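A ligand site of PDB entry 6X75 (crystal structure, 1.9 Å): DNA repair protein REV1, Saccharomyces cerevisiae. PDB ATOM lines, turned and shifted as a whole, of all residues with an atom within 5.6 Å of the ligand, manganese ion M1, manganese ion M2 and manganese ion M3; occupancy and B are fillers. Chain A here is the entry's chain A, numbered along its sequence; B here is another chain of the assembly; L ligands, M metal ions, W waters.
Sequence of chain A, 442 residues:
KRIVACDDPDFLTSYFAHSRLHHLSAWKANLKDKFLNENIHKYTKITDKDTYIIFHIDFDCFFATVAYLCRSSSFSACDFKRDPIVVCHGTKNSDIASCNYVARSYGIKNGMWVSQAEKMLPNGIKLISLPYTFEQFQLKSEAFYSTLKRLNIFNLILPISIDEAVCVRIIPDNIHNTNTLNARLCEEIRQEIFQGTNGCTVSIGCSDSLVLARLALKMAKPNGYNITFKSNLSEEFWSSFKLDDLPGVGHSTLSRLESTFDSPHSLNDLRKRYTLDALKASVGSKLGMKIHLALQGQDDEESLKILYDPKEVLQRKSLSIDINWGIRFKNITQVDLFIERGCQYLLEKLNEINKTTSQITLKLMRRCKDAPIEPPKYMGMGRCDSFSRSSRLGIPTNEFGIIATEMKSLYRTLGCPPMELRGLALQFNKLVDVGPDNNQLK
OH of Tyr 101 sits at hydrogen-bond distance from O11 of the ligand, at 2.8 Å.
An oxygen (O12) of the ligand is in salt-bridge range of the guanidinium group (NH1) of Arg 104.
The guanidinium group (NE) of Arg 20 lies within hydrogen-bond range of an oxygen (O1) of the ligand, 2.8 Å away.
An oxygen (O8) of the ligand sits at hydrogen-bond distance from the side-chain hydroxyl (OG) of Ser 98, at 2.8 Å.
An oxygen (O8) of the ligand lies within hydrogen-bond range of the backbone NH (N) of Phe 62, 3.4 Å away.
An oxygen (O11) of the ligand lies within hydrogen-bond range of the backbone NH (N) of Cys 61.
O11 of the ligand lies within salt-bridge range of NZ of Lys 221, at 3.0 Å.
N of Phe 63 sits at hydrogen-bond distance from O3 of the ligand.
An oxygen (O8) of the ligand lies within hydrogen-bond range of the side-chain amide nitrogen (ND2) of Asn 110 (3.2 Å).
The backbone carbonyl oxygen (O) of Asp 58 is in hydrogen-bond range of the side-chain amino group (NZ) of Lys 221 (3.4 Å).
OP1 of DC 13 of chain B lies close to OG of Ser 161, at 3.3 Å.
N of Asp 163 is in hydrogen-bond range of OG of Ser 161, 3.0 Å away.
The backbone NH of Glu 164 lies close to the side-chain hydroxyl of Ser 161 (3.5 Å).
The side-chain hydroxyl (OH) of Tyr 101 lies within hydrogen-bond range of the guanidinium group (NH1) of Arg 104, at 3.3 Å.
The backbone carbonyl oxygen (O) of Cys 99 lies within hydrogen-bond range of the guanidinium group (NE) of Arg 104.
The backbone NH (N) of Ala 64 lies within hydrogen-bond range of the side-chain hydroxyl (OG) of Ser 98.
OD1 of Asn 110 sits at hydrogen-bond distance from N of Cys 99 (3.1 Å).
The backbone carbonyl oxygen (O) of Ala 97 sits close to a nitrogen (N1) of the ligand, 3.3 Å away.
Leu 24 touches the ligand.
Asp 60 touches the ligand.
CA of Gly 111 touches N3 of the ligand (3.8 Å).
Hydrophobic or aromatic side chains that line the ligand: Leu 24, Phe 62, Phe 63, Ala 97 and Tyr 101.
Within 4 Å of the ligand: Arg 20, Leu 24, Asp 58, Phe 59, Asp 60, Cys 61, Phe 62, Phe 63, Ala 97, Ser 98, Tyr 101, Arg 104, Asn 110, Gly 111, Asp 163, Lys 221 and DC 13 of chain B.
Along chain A the residues within 4 Å of the ligand span positions 20 to 221.
The nearest printed residue that does not touch the ligand is Leu 21 (4.4 Å).
The nearest printed residue that does not touch manganese ion M1 is Arg 214 (4.6 Å).
Merely in contact with manganese ion M2: Ser 161 (3.97 Å).
The nearest printed residue that does not touch manganese ion M2 is DG 12 of chain B (4.3 Å).
Of the 26 residues printed, 3 come within 4 Å of manganese ion M3.
Manganese ion M1 is bound by O6 of the ligand, water W7, water W1, water W8, OP2 of DC 13 of chain B and water W4.
Manganese ion M1 has six donor atoms within binding distance.
Manganese ion M2 is bound by O5 of the ligand (2.1 Å), OD2 of Asp 58 (2.2 Å), OP1 of DC 13 of chain B (2.2 Å), water W7 (2.3 Å), OD1 of Asp 163 (2.3 Å) and OE2 of Glu 164 (2.4 Å).
Manganese ion M3 is bound by the side-chain carboxylate (OD1) of Asp 58, 2.1 Å away.
Manganese ion M3 is bound by O9 of the ligand.
Manganese ion M3 is bound by O of Phe 59, at 2.2 Å.
The side-chain carboxylate (OD2) of Asp 163 binds manganese ion M3.
O5 of the ligand binds manganese ion M3 (2.3 Å).
O13 of the ligand is bound to manganese ion M3 (2.3 Å).
Manganese ion M3 has six donor atoms within binding distance.
Water W4 lies within hydrogen-bond range of OP2 of DG 12 of chain B (2.7 Å) and NH2 of Arg 214 (3.4 Å).
Water W3 bridges the guanidinium group (NH2) of Arg 20 (3.0 Å) and a nitrogen (N3) of the ligand (3.0 Å).
Water W6 bridges the side-chain amide nitrogen of Asn 110 (2.8 Å) and an oxygen (O7) of the ligand (3.4 Å).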
ATOM      1  N   ARG A  20     -29.401  18.234 -22.896  1.00  0.00           N
ATOM      2  CA  ARG A  20     -28.397  19.014 -23.588  1.00  0.00           C
ATOM      3  C   ARG A  20     -27.889  18.308 -24.837  1.00  0.00           C
ATOM      4  O   ARG A  20     -27.577  18.974 -25.831  1.00  0.00           O
ATOM      5  CB  ARG A  20     -27.242  19.389 -22.657  1.00  0.00           C
ATOM      6  CG  ARG A  20     -25.984  18.545 -22.793  1.00  0.00           C
ATOM      7  CD  ARG A  20     -25.991  17.340 -21.863  1.00  0.00           C
ATOM      8  NE  ARG A  20     -24.669  16.715 -21.877  1.00  0.00           N
ATOM      9  CZ  ARG A  20     -24.360  15.541 -21.326  1.00  0.00           C
ATOM     10  NH1 ARG A  20     -25.274  14.830 -20.691  1.00  0.00           N
ATOM     11  NH2 ARG A  20     -23.117  15.079 -21.395  1.00  0.00           N
ATOM     12  N   LEU A  21     -27.866  16.959 -24.834  1.00  0.00           N
ATOM     13  CA  LEU A  21     -27.396  16.279 -26.046  1.00  0.00           C
ATOM     14  C   LEU A  21     -28.406  16.400 -27.184  1.00  0.00           C
ATOM     15  O   LEU A  21     -28.008  16.513 -28.354  1.00  0.00           O
ATOM     16  CB  LEU A  21     -27.068  14.810 -25.767  1.00  0.00           C
ATOM     17  CG  LEU A  21     -25.948  14.541 -24.743  1.00  0.00           C
ATOM     18  CD1 LEU A  21     -25.830  13.071 -24.351  1.00  0.00           C
ATOM     19  CD2 LEU A  21     -24.617  15.038 -25.259  1.00  0.00           C
ATOM     20  N   LEU A  24     -27.649  19.862 -28.585  1.00  0.00           N
ATOM     21  CA  LEU A  24     -26.451  19.846 -29.434  1.00  0.00           C
ATOM     22  C   LEU A  24     -26.764  19.321 -30.830  1.00  0.00           C
ATOM     23  O   LEU A  24     -26.365  19.908 -31.845  1.00  0.00           O
ATOM     24  CB  LEU A  24     -25.344  18.996 -28.798  1.00  0.00           C
ATOM     25  CG  LEU A  24     -24.804  19.505 -27.463  1.00  0.00           C
ATOM     26  CD1 LEU A  24     -23.837  18.505 -26.849  1.00  0.00           C
ATOM     27  CD2 LEU A  24     -24.112  20.840 -27.679  1.00  0.00           C
ATOM     28  N   ASP A  58     -13.038  27.382 -31.823  1.00  0.00           N
ATOM     29  CA  ASP A  58     -13.893  26.674 -30.862  1.00  0.00           C
ATOM     30  C   ASP A  58     -13.946  27.434 -29.533  1.00  0.00           C
ATOM     31  O   ASP A  58     -12.899  27.829 -29.011  1.00  0.00           O
ATOM     32  CB  ASP A  58     -13.342  25.247 -30.670  1.00  0.00           C
ATOM     33  CG  ASP A  58     -14.199  24.418 -29.754  1.00  0.00           C
ATOM     34  OD1 ASP A  58     -14.072  24.573 -28.517  1.00  0.00           O
ATOM     35  OD2 ASP A  58     -14.968  23.589 -30.278  1.00  0.00           O
ATOM     36  N   PHE A  59     -15.148  27.604 -28.981  1.00  0.00           N
ATOM     37  CA  PHE A  59     -15.294  28.255 -27.671  1.00  0.00           C
ATOM     38  C   PHE A  59     -14.592  27.462 -26.564  1.00  0.00           C
ATOM     39  O   PHE A  59     -14.719  26.247 -26.488  1.00  0.00           O
ATOM     40  CB  PHE A  59     -16.766  28.346 -27.260  1.00  0.00           C
ATOM     41  CG  PHE A  59     -17.568  29.429 -27.914  1.00  0.00           C
ATOM     42  CD1 PHE A  59     -18.075  29.270 -29.192  1.00  0.00           C
ATOM     43  CD2 PHE A  59     -17.915  30.579 -27.207  1.00  0.00           C
ATOM     44  CE1 PHE A  59     -18.851  30.237 -29.777  1.00  0.00           C
ATOM     45  CE2 PHE A  59     -18.710  31.547 -27.776  1.00  0.00           C
ATOM     46  CZ  PHE A  59     -19.190  31.383 -29.066  1.00  0.00           C
ATOM     47  N   ASP A  60     -13.921  28.171 -25.661  1.00  0.00           N
ATOM     48  CA  ASP A  60     -13.406  27.526 -24.462  1.00  0.00           C
ATOM     49  C   ASP A  60     -14.545  27.243 -23.498  1.00  0.00           C
ATOM     50  O   ASP A  60     -15.423  28.092 -23.289  1.00  0.00           O
ATOM     51  CB  ASP A  60     -12.343  28.396 -23.791  1.00  0.00           C
ATOM     52  CG  ASP A  60     -11.294  28.887 -24.781  1.00  0.00           C
ATOM     53  OD1 ASP A  60     -10.784  28.042 -25.565  1.00  0.00           O
ATOM     54  OD2 ASP A  60     -10.984  30.088 -24.781  1.00  0.00           O
ATOM     55  N   CYS A  61     -14.518  26.048 -22.892  1.00  0.00           N
ATOM     56  CA  CYS A  61     -15.579  25.469 -22.054  1.00  0.00           C
ATOM     57  C   CYS A  61     -16.908  26.189 -22.237  1.00  0.00           C
ATOM     58  O   CYS A  61     -17.376  26.911 -21.345  1.00  0.00           O
ATOM     59  CB  CYS A  61     -15.162  25.477 -20.570  1.00  0.00           C
ATOM     60  SG  CYS A  61     -14.445  27.061 -20.020  1.00  0.00           S
ATOM     61  N   PHE A  62     -17.505  25.977 -23.408  1.00  0.00           N
ATOM     62  CA  PHE A  62     -18.606  26.811 -23.910  1.00  0.00           C
ATOM     63  C   PHE A  62     -19.755  26.950 -22.919  1.00  0.00           C
ATOM     64  O   PHE A  62     -20.067  28.057 -22.468  1.00  0.00           O
ATOM     65  CB  PHE A  62     -19.085  26.196 -25.212  1.00  0.00           C
ATOM     66  CG  PHE A  62     -20.229  26.939 -25.852  1.00  0.00           C
ATOM     67  CD1 PHE A  62     -20.132  28.272 -26.127  1.00  0.00           C
ATOM     68  CD2 PHE A  62     -21.393  26.262 -26.226  1.00  0.00           C
ATOM     69  CE1 PHE A  62     -21.149  28.949 -26.747  1.00  0.00           C
ATOM     70  CE2 PHE A  62     -22.427  26.914 -26.844  1.00  0.00           C
ATOM     71  CZ  PHE A  62     -22.316  28.265 -27.098  1.00  0.00           C
ATOM     72  N   PHE A  63     -20.426  25.825 -22.580  1.00  0.00           N
ATOM     73  CA  PHE A  63     -21.549  25.908 -21.641  1.00  0.00           C
ATOM     74  C   PHE A  63     -21.126  26.582 -20.328  1.00  0.00           C
ATOM     75  O   PHE A  63     -21.865  27.408 -19.785  1.00  0.00           O
ATOM     76  CB  PHE A  63     -22.111  24.524 -21.333  1.00  0.00           C
ATOM     77  CG  PHE A  63     -22.993  23.931 -22.421  1.00  0.00           C
ATOM     78  CD1 PHE A  63     -23.054  24.486 -23.705  1.00  0.00           C
ATOM     79  CD2 PHE A  63     -23.761  22.802 -22.150  1.00  0.00           C
ATOM     80  CE1 PHE A  63     -23.868  23.919 -24.684  1.00  0.00           C
ATOM     81  CE2 PHE A  63     -24.575  22.224 -23.116  1.00  0.00           C
ATOM     82  CZ  PHE A  63     -24.622  22.772 -24.384  1.00  0.00           C
ATOM     83  N   ALA A  64     -19.956  26.216 -19.810  1.00  0.00           N
ATOM     84  CA  ALA A  64     -19.527  26.778 -18.520  1.00  0.00           C
ATOM     85  C   ALA A  64     -19.351  28.291 -18.616  1.00  0.00           C
ATOM     86  O   ALA A  64     -19.833  29.041 -17.768  1.00  0.00           O
ATOM     87  CB  ALA A  64     -18.232  26.115 -18.062  1.00  0.00           C
ATOM     88  N   ILE A  96     -21.608  16.050 -16.110  1.00  0.00           N
ATOM     89  CA  ILE A  96     -21.031  17.380 -16.240  1.00  0.00           C
ATOM     90  C   ILE A  96     -20.968  17.676 -17.733  1.00  0.00           C
ATOM     91  O   ILE A  96     -20.219  17.040 -18.472  1.00  0.00           O
ATOM     92  CB  ILE A  96     -19.641  17.467 -15.585  1.00  0.00           C
ATOM     93  CG1 ILE A  96     -19.794  17.502 -14.064  1.00  0.00           C
ATOM     94  CG2 ILE A  96     -18.866  18.676 -16.110  1.00  0.00           C
ATOM     95  CD1 ILE A  96     -18.518  17.097 -13.357  1.00  0.00           C
ATOM     96  N   ALA A  97     -21.813  18.601 -18.187  1.00  0.00           N
ATOM     97  CA  ALA A  97     -21.830  18.917 -19.611  1.00  0.00           C
ATOM     98  C   ALA A  97     -20.574  19.672 -20.001  1.00  0.00           C
ATOM     99  O   ALA A  97     -19.972  19.386 -21.043  1.00  0.00           O
ATOM    100  CB  ALA A  97     -23.081  19.716 -19.953  1.00  0.00           C
ATOM    101  N   SER A  98     -20.173  20.626 -19.173  1.00  0.00           N
ATOM    102  CA  SER A  98     -18.978  21.419 -19.430  1.00  0.00           C
ATOM    103  C   SER A  98     -18.395  21.819 -18.086  1.00  0.00           C
ATOM    104  O   SER A  98     -19.115  22.032 -17.101  1.00  0.00           O
ATOM    105  CB  SER A  98     -19.309  22.639 -20.298  1.00  0.00           C
ATOM    106  OG  SER A  98     -18.170  23.460 -20.503  1.00  0.00           O
ATOM    107  N   CYS A  99     -17.088  21.894 -18.030  1.00  0.00           N
ATOM    108  CA  CYS A  99     -16.418  22.369 -16.842  1.00  0.00           C
ATOM    109  C   CYS A  99     -15.308  23.322 -17.228  1.00  0.00           C
ATOM    110  O   CYS A  99     -14.707  23.199 -18.302  1.00  0.00           O
ATOM    111  CB  CYS A  99     -15.908  21.187 -16.019  1.00  0.00           C
ATOM    112  SG  CYS A  99     -14.637  20.236 -16.905  1.00  0.00           S
ATOM    113  N   TYR A 101     -11.693  25.624 -16.708  1.00  0.00           N
ATOM    114  CA  TYR A 101     -10.331  25.120 -16.678  1.00  0.00           C
ATOM    115  C   TYR A 101      -9.787  25.007 -15.256  1.00  0.00           C
ATOM    116  O   TYR A 101      -8.921  24.168 -15.021  1.00  0.00           O
ATOM    117  CB  TYR A 101      -9.458  25.999 -17.593  1.00  0.00           C
ATOM    118  CG  TYR A 101      -9.608  25.500 -19.014  1.00  0.00           C
ATOM    119  CD1 TYR A 101     -10.758  25.810 -19.769  1.00  0.00           C
ATOM    120  CD2 TYR A 101      -8.666  24.639 -19.588  1.00  0.00           C
ATOM    121  CE1 TYR A 101     -10.929  25.322 -21.071  1.00  0.00           C
ATOM    122  CE2 TYR A 101      -8.829  24.146 -20.886  1.00  0.00           C
ATOM    123  CZ  TYR A 101      -9.963  24.485 -21.611  1.00  0.00           C
ATOM    124  OH  TYR A 101     -10.134  24.010 -22.895  1.00  0.00           O
ATOM    125  N   ARG A 104     -10.726  21.593 -14.485  1.00  0.00           N
ATOM    126  CA  ARG A 104      -9.910  20.622 -15.204  1.00  0.00           C
ATOM    127  C   ARG A 104      -8.522  20.470 -14.584  1.00  0.00           C
ATOM    128  O   ARG A 104      -7.896  19.405 -14.733  1.00  0.00           O
ATOM    129  CB  ARG A 104      -9.795  21.028 -16.668  1.00  0.00           C
ATOM    130  CG  ARG A 104     -11.164  21.139 -17.357  1.00  0.00           C
ATOM    131  CD  ARG A 104     -11.061  21.398 -18.851  1.00  0.00           C
ATOM    132  NE  ARG A 104     -12.381  21.726 -19.390  1.00  0.00           N
ATOM    133  CZ  ARG A 104     -12.697  21.755 -20.684  1.00  0.00           C
ATOM    134  NH1 ARG A 104     -11.780  21.460 -21.603  1.00  0.00           N
ATOM    135  NH2 ARG A 104     -13.953  22.071 -21.041  1.00  0.00           N
ATOM    136  N   ASN A 110     -15.341  16.931 -19.114  1.00  0.00           N
ATOM    137  CA  ASN A 110     -16.710  16.894 -19.605  1.00  0.00           C
ATOM    138  C   ASN A 110     -17.184  15.449 -19.641  1.00  0.00           C
ATOM    139  O   ASN A 110     -16.435  14.548 -20.023  1.00  0.00           O
ATOM    140  CB  ASN A 110     -16.807  17.484 -21.015  1.00  0.00           C
ATOM    141  CG  ASN A 110     -16.537  18.980 -21.038  1.00  0.00           C
ATOM    142  OD1 ASN A 110     -16.452  19.629 -20.005  1.00  0.00           O
ATOM    143  ND2 ASN A 110     -16.434  19.534 -22.244  1.00  0.00           N
ATOM    144  N   GLY A 111     -18.444  15.227 -19.261  1.00  0.00           N
ATOM    145  CA  GLY A 111     -19.023  13.906 -19.317  1.00  0.00           C
ATOM    146  C   GLY A 111     -18.878  13.108 -18.042  1.00  0.00           C
ATOM    147  O   GLY A 111     -19.545  12.070 -17.907  1.00  0.00           O
ATOM    148  N   SER A 161     -20.314  22.598 -34.896  1.00  0.00           N
ATOM    149  CA  SER A 161     -21.247  22.446 -33.801  1.00  0.00           C
ATOM    150  C   SER A 161     -21.742  23.817 -33.395  1.00  0.00           C
ATOM    151  O   SER A 161     -21.402  24.840 -34.025  1.00  0.00           O
ATOM    152  CB  SER A 161     -20.582  21.729 -32.616  1.00  0.00           C
ATOM    153  OG  SER A 161     -19.764  22.618 -31.869  1.00  0.00           O
ATOM    154  N   ILE A 162     -22.567  23.829 -32.355  1.00  0.00           N
ATOM    155  CA  ILE A 162     -22.974  25.072 -31.699  1.00  0.00           C
ATOM    156  C   ILE A 162     -21.780  25.952 -31.347  1.00  0.00           C
ATOM    157  O   ILE A 162     -21.890  27.190 -31.356  1.00  0.00           O
ATOM    158  CB  ILE A 162     -23.822  24.737 -30.447  1.00  0.00           C
ATOM    159  CG1 ILE A 162     -24.456  26.008 -29.884  1.00  0.00           C
ATOM    160  CG2 ILE A 162     -22.976  24.055 -29.350  1.00  0.00           C
ATOM    161  CD1 ILE A 162     -25.609  26.548 -30.752  1.00  0.00           C
ATOM    162  N   ASP A 163     -20.621  25.376 -31.003  1.00  0.00           N
ATOM    163  CA  ASP A 163     -19.532  26.193 -30.493  1.00  0.00           C
ATOM    164  C   ASP A 163     -18.282  26.120 -31.367  1.00  0.00           C
ATOM    165  O   ASP A 163     -17.185  26.431 -30.905  1.00  0.00           O
ATOM    166  CB  ASP A 163     -19.215  25.847 -29.031  1.00  0.00           C
ATOM    167  CG  ASP A 163     -18.166  24.744 -28.891  1.00  0.00           C
ATOM    168  OD1 ASP A 163     -18.195  23.730 -29.632  1.00  0.00           O
ATOM    169  OD2 ASP A 163     -17.254  24.921 -28.040  1.00  0.00           O
ATOM    170  N   GLU A 164     -18.413  25.728 -32.629  1.00  0.00           N
ATOM    171  CA  GLU A 164     -17.206  25.329 -33.333  1.00  0.00           C
ATOM    172  C   GLU A 164     -17.409  25.424 -34.827  1.00  0.00           C
ATOM    173  O   GLU A 164     -18.426  24.940 -35.338  1.00  0.00           O
ATOM    174  CB  GLU A 164     -16.861  23.895 -32.930  1.00  0.00           C
ATOM    175  CG  GLU A 164     -15.649  23.308 -33.584  1.00  0.00           C
ATOM    176  CD  GLU A 164     -15.316  21.972 -32.963  1.00  0.00           C
ATOM    177  OE1 GLU A 164     -14.418  21.284 -33.487  1.00  0.00           O
ATOM    178  OE2 GLU A 164     -15.978  21.608 -31.952  1.00  0.00           O
ATOM    179  N   ARG A 214      -6.974  20.816 -36.092  1.00  0.00           N
ATOM    180  CA  ARG A 214      -7.647  20.260 -34.916  1.00  0.00           C
ATOM    181  C   ARG A 214      -6.660  20.036 -33.780  1.00  0.00           C
ATOM    182  O   ARG A 214      -6.947  20.360 -32.617  1.00  0.00           O
ATOM    183  CB  ARG A 214      -8.355  18.957 -35.279  1.00  0.00           C
ATOM    184  CG  ARG A 214      -9.051  18.287 -34.091  1.00  0.00           C
ATOM    185  CD  ARG A 214     -10.234  19.126 -33.590  1.00  0.00           C
ATOM    186  NE  ARG A 214     -10.813  18.612 -32.345  1.00  0.00           N
ATOM    187  CZ  ARG A 214     -10.417  18.976 -31.131  1.00  0.00           C
ATOM    188  NH1 ARG A 214      -9.425  19.858 -30.996  1.00  0.00           N
ATOM    189  NH2 ARG A 214     -10.998  18.460 -30.057  1.00  0.00           N
ATOM    190  N   LYS A 221      -5.569  25.673 -26.566  1.00  0.00           N
ATOM    191  CA  LYS A 221      -6.500  25.909 -25.464  1.00  0.00           C
ATOM    192  C   LYS A 221      -5.764  25.954 -24.125  1.00  0.00           C
ATOM    193  O   LYS A 221      -4.766  25.264 -23.936  1.00  0.00           O
ATOM    194  CB  LYS A 221      -7.566  24.817 -25.426  1.00  0.00           C
ATOM    195  CG  LYS A 221      -8.736  25.130 -26.304  1.00  0.00           C
ATOM    196  CD  LYS A 221      -9.683  23.960 -26.448  1.00  0.00           C
ATOM    197  CE  LYS A 221     -10.806  24.330 -27.414  1.00  0.00           C
ATOM    198  NZ  LYS A 221     -11.619  25.472 -26.899  1.00  0.00           N
ATOM    199  P    DG B  12     -14.691  16.155 -33.413  1.00  0.00           P
ATOM    200  OP1  DG B  12     -13.591  17.107 -33.748  1.00  0.00           O
ATOM    201  OP2  DG B  12     -14.645  15.419 -32.139  1.00  0.00           O
ATOM    202  O5'  DG B  12     -16.034  16.996 -33.513  1.00  0.00           O
ATOM    203  C5'  DG B  12     -16.917  16.987 -32.452  1.00  0.00           C
ATOM    204  C4'  DG B  12     -18.235  17.573 -32.875  1.00  0.00           C
ATOM    205  O4'  DG B  12     -18.912  16.610 -33.736  1.00  0.00           O
ATOM    206  C3'  DG B  12     -19.191  17.807 -31.716  1.00  0.00           C
ATOM    207  O3'  DG B  12     -19.060  19.127 -31.197  1.00  0.00           O
ATOM    208  C2'  DG B  12     -20.548  17.591 -32.392  1.00  0.00           C
ATOM    209  C1'  DG B  12     -20.221  16.381 -33.250  1.00  0.00           C
ATOM    210  N9   DG B  12     -20.237  15.134 -32.472  1.00  0.00           N
ATOM    211  C8   DG B  12     -19.162  14.355 -32.066  1.00  0.00           C
ATOM    212  N7   DG B  12     -19.520  13.328 -31.344  1.00  0.00           N
ATOM    213  C5   DG B  12     -20.905  13.431 -31.265  1.00  0.00           C
ATOM    214  C6   DG B  12     -21.871  12.600 -30.614  1.00  0.00           C
ATOM    215  O6   DG B  12     -21.682  11.557 -29.948  1.00  0.00           O
ATOM    216  N1   DG B  12     -23.167  13.086 -30.791  1.00  0.00           N
ATOM    217  C2   DG B  12     -23.500  14.225 -31.510  1.00  0.00           C
ATOM    218  N2   DG B  12     -24.796  14.531 -31.588  1.00  0.00           N
ATOM    219  N3   DG B  12     -22.620  14.984 -32.114  1.00  0.00           N
ATOM    220  C4   DG B  12     -21.357  14.541 -31.946  1.00  0.00           C
ATOM    221  P    DC B  13     -18.140  19.431 -29.906  1.00  0.00           P
ATOM    222  OP1  DC B  13     -18.299  20.861 -29.539  1.00  0.00           O
ATOM    223  OP2  DC B  13     -16.787  18.925 -30.232  1.00  0.00           O
ATOM    224  O5'  DC B  13     -18.703  18.511 -28.733  1.00  0.00           O
ATOM    225  C5'  DC B  13     -20.088  18.478 -28.437  1.00  0.00           C
ATOM    226  C4'  DC B  13     -20.595  17.038 -28.388  1.00  0.00           C
ATOM    227  O4'  DC B  13     -19.681  16.160 -29.094  1.00  0.00           O
ATOM    228  C3'  DC B  13     -20.756  16.440 -26.994  1.00  0.00           C
ATOM    229  O3'  DC B  13     -22.020  15.796 -26.892  1.00  0.00           O
ATOM    230  C2'  DC B  13     -19.606  15.423 -26.913  1.00  0.00           C
ATOM    231  C1'  DC B  13     -19.544  14.978 -28.353  1.00  0.00           C
ATOM    232  N1   DC B  13     -18.275  14.308 -28.735  1.00  0.00           N
ATOM    233  C2   DC B  13     -18.065  12.966 -28.383  1.00  0.00           C
ATOM    234  O2   DC B  13     -18.926  12.366 -27.719  1.00  0.00           O
ATOM    235  N3   DC B  13     -16.909  12.354 -28.768  1.00  0.00           N
ATOM    236  C4   DC B  13     -16.006  13.030 -29.483  1.00  0.00           C
ATOM    237  N4   DC B  13     -14.882  12.394 -29.828  1.00  0.00           N
ATOM    238  C5   DC B  13     -16.203  14.398 -29.860  1.00  0.00           C
ATOM    239  C6   DC B  13     -17.346  14.989 -29.476  1.00  0.00           C
HETATM  240  N1  LIG L   1     -20.770  18.934 -24.166  1.00  0.00           N
HETATM  241  C1  LIG L   1     -21.658  18.015 -23.417  1.00  0.00           C
HETATM  242  N2  LIG L   1     -21.169  16.681 -23.010  1.00  0.00           N
HETATM  243  C2  LIG L   1     -19.830  16.279 -23.334  1.00  0.00           C
HETATM  244  C3  LIG L   1     -18.921  17.208 -24.091  1.00  0.00           C
HETATM  245  C4  LIG L   1     -19.421  18.536 -24.510  1.00  0.00           C
HETATM  246  O1  LIG L   1     -22.752  18.389 -23.155  1.00  0.00           O
HETATM  247  N3  LIG L   1     -19.385  14.971 -22.936  1.00  0.00           N
HETATM  248  C5  LIG L   1     -21.349  20.212 -24.498  1.00  0.00           C
HETATM  249  C6  LIG L   1     -20.965  21.103 -23.573  1.00  0.00           C
HETATM  250  C7  LIG L   1     -19.707  21.868 -24.244  1.00  0.00           C
HETATM  251  C8  LIG L   1     -20.147  22.045 -25.536  1.00  0.00           C
HETATM  252  O2  LIG L   1     -20.768  20.703 -25.865  1.00  0.00           O
HETATM  253  O3  LIG L   1     -19.474  23.094 -23.544  1.00  0.00           O
HETATM  254  C9  LIG L   1     -19.034  22.163 -26.550  1.00  0.00           C
HETATM  255  O4  LIG L   1     -18.325  20.942 -26.529  1.00  0.00           O
HETATM  256  P1  LIG L   1     -16.690  21.039 -26.600  1.00  0.00           P
HETATM  257  O5  LIG L   1     -16.281  22.155 -27.577  1.00  0.00           O
HETATM  258  O6  LIG L   1     -16.109  19.688 -26.976  1.00  0.00           O
HETATM  259  O7  LIG L   1     -16.115  21.333 -25.039  1.00  0.00           O
HETATM  260  P2  LIG L   1     -16.075  22.725 -24.211  1.00  0.00           P
HETATM  261  O8  LIG L   1     -16.916  22.637 -22.925  1.00  0.00           O
HETATM  262  O9  LIG L   1     -16.441  23.903 -25.142  1.00  0.00           O
HETATM  263  O10 LIG L   1     -14.513  22.884 -23.656  1.00  0.00           O
HETATM  264  P3  LIG L   1     -13.183  23.035 -24.639  1.00  0.00           P
HETATM  265  O11 LIG L   1     -12.511  24.384 -24.276  1.00  0.00           O
HETATM  266  O12 LIG L   1     -12.269  21.851 -24.356  1.00  0.00           O
HETATM  267  O13 LIG L   1     -13.618  23.031 -26.076  1.00  0.00           O
HETATM  268 MN    MN M   1     -15.214  18.509 -28.304  1.00  0.00          MN
HETATM  269 MN    MN M   2     -16.465  22.148 -29.713  1.00  0.00          MN
HETATM  270 MN    MN M   3     -15.419  24.174 -26.971  1.00  0.00          MN
HETATM  271  O   HOH W   1     -15.944  16.734 -26.733  1.00  0.00           O
HETATM  272  O   HOH W   2     -16.863  13.975 -23.943  1.00  0.00           O
HETATM  273  O   HOH W   3     -21.358  12.833 -22.248  1.00  0.00           O
HETATM  274  O   HOH W   4     -14.032  17.007 -30.079  1.00  0.00           O
HETATM  275  O   HOH W   5     -13.086  19.246 -24.145  1.00  0.00           O
HETATM  276  O   HOH W   6     -15.647  17.987 -24.395  1.00  0.00           O
HETATM  277  O   HOH W   7     -14.906  20.515 -29.701  1.00  0.00           O
HETATM  278  O   HOH W   8     -12.962  18.803 -27.217  1.00  0.00           O
HETATM  279  O   HOH W   9     -10.217  20.657 -25.432  1.00  0.00           O
HETATM  280  O   HOH W  10     -12.930  21.317 -27.997  1.00  0.00           O
